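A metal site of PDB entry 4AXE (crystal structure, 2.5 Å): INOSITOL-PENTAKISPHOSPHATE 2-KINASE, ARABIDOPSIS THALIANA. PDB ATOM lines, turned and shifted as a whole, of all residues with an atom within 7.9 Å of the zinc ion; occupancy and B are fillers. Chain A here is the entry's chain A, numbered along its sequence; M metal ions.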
ATOM      1  N   GLU A 321     -35.589   9.866   1.074  1.00  0.00           N
ATOM      2  CA  GLU A 321     -34.838  10.161  -0.152  1.00  0.00           C
ATOM      3  C   GLU A 321     -34.106  11.502  -0.097  1.00  0.00           C
ATOM      4  O   GLU A 321     -33.034  11.657  -0.701  1.00  0.00           O
ATOM      5  CB  GLU A 321     -35.741  10.143  -1.374  1.00  0.00           C
ATOM      6  CG  GLU A 321     -35.898   8.777  -2.023  1.00  0.00           C
ATOM      7  CD  GLU A 321     -36.451   8.878  -3.426  1.00  0.00           C
ATOM      8  OE1 GLU A 321     -35.714   9.327  -4.328  1.00  0.00           O
ATOM      9  OE2 GLU A 321     -37.617   8.498  -3.650  1.00  0.00           O
ATOM     10  N   GLY A 322     -34.700  12.453   0.615  1.00  0.00           N
ATOM     11  CA  GLY A 322     -34.079  13.764   0.826  1.00  0.00           C
ATOM     12  C   GLY A 322     -33.256  13.783   2.100  1.00  0.00           C
ATOM     13  O   GLY A 322     -32.125  14.281   2.100  1.00  0.00           O
ATOM     14  N   ILE A 324     -31.714  11.453   3.817  1.00  0.00           N
ATOM     15  CA  ILE A 324     -30.478  10.648   3.816  1.00  0.00           C
ATOM     16  C   ILE A 324     -29.236  11.454   3.441  1.00  0.00           C
ATOM     17  O   ILE A 324     -28.124  11.115   3.856  1.00  0.00           O
ATOM     18  CB  ILE A 324     -30.627   9.381   2.912  1.00  0.00           C
ATOM     19  CG1 ILE A 324     -29.483   8.385   3.160  1.00  0.00           C
ATOM     20  CG2 ILE A 324     -30.719   9.755   1.441  1.00  0.00           C
ATOM     21  CD1 ILE A 324     -29.589   7.605   4.454  1.00  0.00           C
ATOM     22  N   HIS A 325     -29.429  12.526   2.679  1.00  0.00           N
ATOM     23  CA  HIS A 325     -28.323  13.396   2.284  1.00  0.00           C
ATOM     24  C   HIS A 325     -27.841  14.210   3.439  1.00  0.00           C
ATOM     25  O   HIS A 325     -26.626  14.362   3.630  1.00  0.00           O
ATOM     26  CB  HIS A 325     -28.718  14.287   1.100  1.00  0.00           C
ATOM     27  CG  HIS A 325     -29.135  13.525  -0.129  1.00  0.00           C
ATOM     28  ND1 HIS A 325     -28.273  12.785  -0.855  1.00  0.00           N
ATOM     29  CD2 HIS A 325     -30.369  13.387  -0.755  1.00  0.00           C
ATOM     30  CE1 HIS A 325     -28.920  12.210  -1.883  1.00  0.00           C
ATOM     31  NE2 HIS A 325     -30.204  12.585  -1.823  1.00  0.00           N
ATOM     32  N   CYS A 326     -28.772  14.719   4.235  1.00  0.00           N
ATOM     33  CA  CYS A 326     -28.448  15.486   5.446  1.00  0.00           C
ATOM     34  C   CYS A 326     -27.714  14.608   6.458  1.00  0.00           C
ATOM     35  O   CYS A 326     -26.794  15.074   7.131  1.00  0.00           O
ATOM     36  CB  CYS A 326     -29.705  16.075   6.071  1.00  0.00           C
ATOM     37  SG  CYS A 326     -30.652  17.158   4.977  1.00  0.00           S
ATOM     38  N   TYR A 328     -25.633  12.034   5.885  1.00  0.00           N
ATOM     39  CA  TYR A 328     -24.231  11.838   5.512  1.00  0.00           C
ATOM     40  C   TYR A 328     -23.381  13.076   5.710  1.00  0.00           C
ATOM     41  O   TYR A 328     -22.175  12.981   5.900  1.00  0.00           O
ATOM     42  CB  TYR A 328     -24.104  11.297   4.079  1.00  0.00           C
ATOM     43  CG  TYR A 328     -24.334   9.801   3.983  1.00  0.00           C
ATOM     44  CD1 TYR A 328     -23.411   8.889   4.481  1.00  0.00           C
ATOM     45  CD2 TYR A 328     -25.503   9.309   3.406  1.00  0.00           C
ATOM     46  CE1 TYR A 328     -23.632   7.528   4.400  1.00  0.00           C
ATOM     47  CE2 TYR A 328     -25.736   7.942   3.327  1.00  0.00           C
ATOM     48  CZ  TYR A 328     -24.796   7.059   3.824  1.00  0.00           C
ATOM     49  OH  TYR A 328     -25.024   5.709   3.730  1.00  0.00           O
ATOM     50  N   ASP A 329     -24.024  14.241   5.689  1.00  0.00           N
ATOM     51  CA  ASP A 329     -23.348  15.491   6.022  1.00  0.00           C
ATOM     52  C   ASP A 329     -23.031  15.568   7.519  1.00  0.00           C
ATOM     53  O   ASP A 329     -21.993  16.109   7.907  1.00  0.00           O
ATOM     54  CB  ASP A 329     -24.194  16.703   5.603  1.00  0.00           C
ATOM     55  CG  ASP A 329     -24.105  16.986   4.105  1.00  0.00           C
ATOM     56  OD1 ASP A 329     -23.159  16.506   3.445  1.00  0.00           O
ATOM     57  OD2 ASP A 329     -25.002  17.691   3.596  1.00  0.00           O
ATOM     58  N   GLN A 333     -19.337  12.096   5.993  1.00  0.00           N
ATOM     59  CA  GLN A 333     -18.941  11.138   4.964  1.00  0.00           C
ATOM     60  C   GLN A 333     -19.431  11.617   3.590  1.00  0.00           C
ATOM     61  O   GLN A 333     -20.527  12.179   3.498  1.00  0.00           O
ATOM     62  CB  GLN A 333     -19.513   9.740   5.250  1.00  0.00           C
ATOM     63  CG  GLN A 333     -19.196   9.161   6.622  1.00  0.00           C
ATOM     64  CD  GLN A 333     -17.732   8.784   6.801  1.00  0.00           C
ATOM     65  OE1 GLN A 333     -17.025   8.489   5.831  1.00  0.00           O
ATOM     66  NE2 GLN A 333     -17.289   8.780   8.051  1.00  0.00           N
ATOM     67  N   PRO A 334     -18.618  11.405   2.534  1.00  0.00           N
ATOM     68  CA  PRO A 334     -19.073  11.644   1.165  1.00  0.00           C
ATOM     69  C   PRO A 334     -20.325  10.830   0.848  1.00  0.00           C
ATOM     70  O   PRO A 334     -20.412   9.649   1.209  1.00  0.00           O
ATOM     71  CB  PRO A 334     -17.893  11.177   0.317  1.00  0.00           C
ATOM     72  CG  PRO A 334     -16.709  11.386   1.196  1.00  0.00           C
ATOM     73  CD  PRO A 334     -17.181  11.058   2.583  1.00  0.00           C
ATOM     74  N   CYS A 335     -21.298  11.458   0.182  1.00  0.00           N
ATOM     75  CA  CYS A 335     -22.601  10.855  -0.074  1.00  0.00           C
ATOM     76  C   CYS A 335     -22.563   9.805  -1.193  1.00  0.00           C
ATOM     77  O   CYS A 335     -22.255  10.143  -2.339  1.00  0.00           O
ATOM     78  CB  CYS A 335     -23.643  11.930  -0.387  1.00  0.00           C
ATOM     79  SG  CYS A 335     -25.332  11.318  -0.563  1.00  0.00           S
ATOM     80  N   PRO A 336     -22.870   8.530  -0.862  1.00  0.00           N
ATOM     81  CA  PRO A 336     -22.873   7.455  -1.867  1.00  0.00           C
ATOM     82  C   PRO A 336     -24.088   7.473  -2.803  1.00  0.00           C
ATOM     83  O   PRO A 336     -24.188   6.624  -3.694  1.00  0.00           O
ATOM     84  CB  PRO A 336     -22.879   6.188  -1.001  1.00  0.00           C
ATOM     85  CG  PRO A 336     -23.561   6.594   0.260  1.00  0.00           C
ATOM     86  CD  PRO A 336     -23.194   8.043   0.486  1.00  0.00           C
ATOM     87  N   ILE A 337     -24.987   8.446  -2.616  1.00  0.00           N
ATOM     88  CA  ILE A 337     -26.186   8.566  -3.448  1.00  0.00           C
ATOM     89  C   ILE A 337     -25.972   9.590  -4.579  1.00  0.00           C
ATOM     90  O   ILE A 337     -26.317   9.336  -5.729  1.00  0.00           O
ATOM     91  CB  ILE A 337     -27.446   8.899  -2.609  1.00  0.00           C
ATOM     92  CG1 ILE A 337     -27.710   7.820  -1.558  1.00  0.00           C
ATOM     93  CG2 ILE A 337     -28.671   9.038  -3.499  1.00  0.00           C
ATOM     94  CD1 ILE A 337     -27.062   8.069  -0.207  1.00  0.00           C
ATOM     95  N   CYS A 338     -25.399  10.747  -4.225  1.00  0.00           N
ATOM     96  CA  CYS A 338     -25.090  11.790  -5.200  1.00  0.00           C
ATOM     97  C   CYS A 338     -23.986  11.374  -6.174  1.00  0.00           C
ATOM     98  O   CYS A 338     -23.119  10.560  -5.832  1.00  0.00           O
ATOM     99  CB  CYS A 338     -24.706  13.094  -4.497  1.00  0.00           C
ATOM    100  SG  CYS A 338     -26.073  13.947  -3.674  1.00  0.00           S
ATOM    101  N   PRO A 343     -26.687  13.538  -9.480  1.00  0.00           N
ATOM    102  CA  PRO A 343     -27.399  14.298  -8.448  1.00  0.00           C
ATOM    103  C   PRO A 343     -28.464  15.243  -8.996  1.00  0.00           C
ATOM    104  O   PRO A 343     -28.391  15.655 -10.157  1.00  0.00           O
ATOM    105  CB  PRO A 343     -26.274  15.112  -7.783  1.00  0.00           C
ATOM    106  CG  PRO A 343     -24.988  14.551  -8.289  1.00  0.00           C
ATOM    107  CD  PRO A 343     -25.308  14.008  -9.651  1.00  0.00           C
ATOM    108  N   LEU A 344     -29.453  15.554  -8.159  1.00  0.00           N
ATOM    109  CA  LEU A 344     -30.474  16.550  -8.480  1.00  0.00           C
ATOM    110  C   LEU A 344     -30.115  17.900  -7.849  1.00  0.00           C
ATOM    111  O   LEU A 344     -29.336  17.958  -6.889  1.00  0.00           O
ATOM    112  CB  LEU A 344     -31.852  16.099  -7.998  1.00  0.00           C
ATOM    113  CG  LEU A 344     -32.420  14.754  -8.481  1.00  0.00           C
ATOM    114  CD1 LEU A 344     -33.639  14.378  -7.662  1.00  0.00           C
ATOM    115  CD2 LEU A 344     -32.752  14.779  -9.967  1.00  0.00           C
ATOM    116  N   GLU A 347     -30.949  18.059  -4.217  1.00  0.00           N
ATOM    117  CA  GLU A 347     -29.979  17.338  -3.391  1.00  0.00           C
ATOM    118  C   GLU A 347     -28.766  18.196  -3.042  1.00  0.00           C
ATOM    119  O   GLU A 347     -28.310  18.213  -1.901  1.00  0.00           O
ATOM    120  CB  GLU A 347     -29.518  16.057  -4.079  1.00  0.00           C
ATOM    121  CG  GLU A 347     -30.628  15.026  -4.300  1.00  0.00           C
ATOM    122  CD  GLU A 347     -30.180  13.827  -5.125  1.00  0.00           C
ATOM    123  OE1 GLU A 347     -29.034  13.824  -5.638  1.00  0.00           O
ATOM    124  OE2 GLU A 347     -30.974  12.870  -5.264  1.00  0.00           O
ATOM    125  N   LEU A 348     -28.256  18.923  -4.041  1.00  0.00           N
ATOM    126  CA  LEU A 348     -27.057  19.749  -3.879  1.00  0.00           C
ATOM    127  C   LEU A 348     -27.298  20.965  -2.992  1.00  0.00           C
ATOM    128  O   LEU A 348     -26.393  21.420  -2.296  1.00  0.00           O
ATOM    129  CB  LEU A 348     -26.518  20.192  -5.249  1.00  0.00           C
ATOM    130  CG  LEU A 348     -26.104  19.092  -6.241  1.00  0.00           C
ATOM    131  CD1 LEU A 348     -25.918  19.677  -7.621  1.00  0.00           C
ATOM    132  CD2 LEU A 348     -24.845  18.371  -5.787  1.00  0.00           C
ATOM    133  N   LEU A 350     -29.372  20.945  -0.450  1.00  0.00           N
ATOM    134  CA  LEU A 350     -29.394  20.392   0.908  1.00  0.00           C
ATOM    135  C   LEU A 350     -28.002  20.273   1.509  1.00  0.00           C
ATOM    136  O   LEU A 350     -27.816  20.493   2.708  1.00  0.00           O
ATOM    137  CB  LEU A 350     -30.069  19.022   0.927  1.00  0.00           C
ATOM    138  CG  LEU A 350     -31.574  18.880   0.683  1.00  0.00           C
ATOM    139  CD1 LEU A 350     -31.943  17.411   0.587  1.00  0.00           C
ATOM    140  CD2 LEU A 350     -32.396  19.571   1.767  1.00  0.00           C
ATOM    141  N   HIS A 351     -27.019  19.925   0.678  1.00  0.00           N
ATOM    142  CA  HIS A 351     -25.625  19.865   1.116  1.00  0.00           C
ATOM    143  C   HIS A 351     -25.053  21.225   1.368  1.00  0.00           C
ATOM    144  O   HIS A 351     -24.053  21.366   2.076  1.00  0.00           O
ATOM    145  CB  HIS A 351     -24.777  19.083   0.122  1.00  0.00           C
ATOM    146  CG  HIS A 351     -25.039  17.589   0.133  1.00  0.00           C
ATOM    147  ND1 HIS A 351     -24.409  16.757   0.973  1.00  0.00           N
ATOM    148  CD2 HIS A 351     -25.898  16.800  -0.631  1.00  0.00           C
ATOM    149  CE1 HIS A 351     -24.840  15.499   0.766  1.00  0.00           C
ATOM    150  NE2 HIS A 351     -25.751  15.528  -0.214  1.00  0.00           N
HETATM  151 ZN    ZN M   1     -26.268  13.568  -1.225  1.00  0.00          ZN
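A ring nitrogen (NE2) of His 325 lies close to the backbone carbonyl oxygen (O) of Glu 321, at 3.2 Å.
ND1 of His 351 lies within hydrogen-bond range of OD1 of Asp 329 (2.8 Å).
SG of Cys 338 lies close to OE1 of Glu 347.
The side-chain sulfur of Cys 335 lies close to the backbone NH of Ile 337 (3.5 Å).
Within 4 Å of the zinc ion: His 325, Cys 335, Cys 338 and His 351.
The zinc ion is bound by a ring nitrogen (ND1) of His 325, a ring nitrogen (NE2) of His 351, the side-chain sulfur of Cys 338 and the side-chain sulfur of Cys 335.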
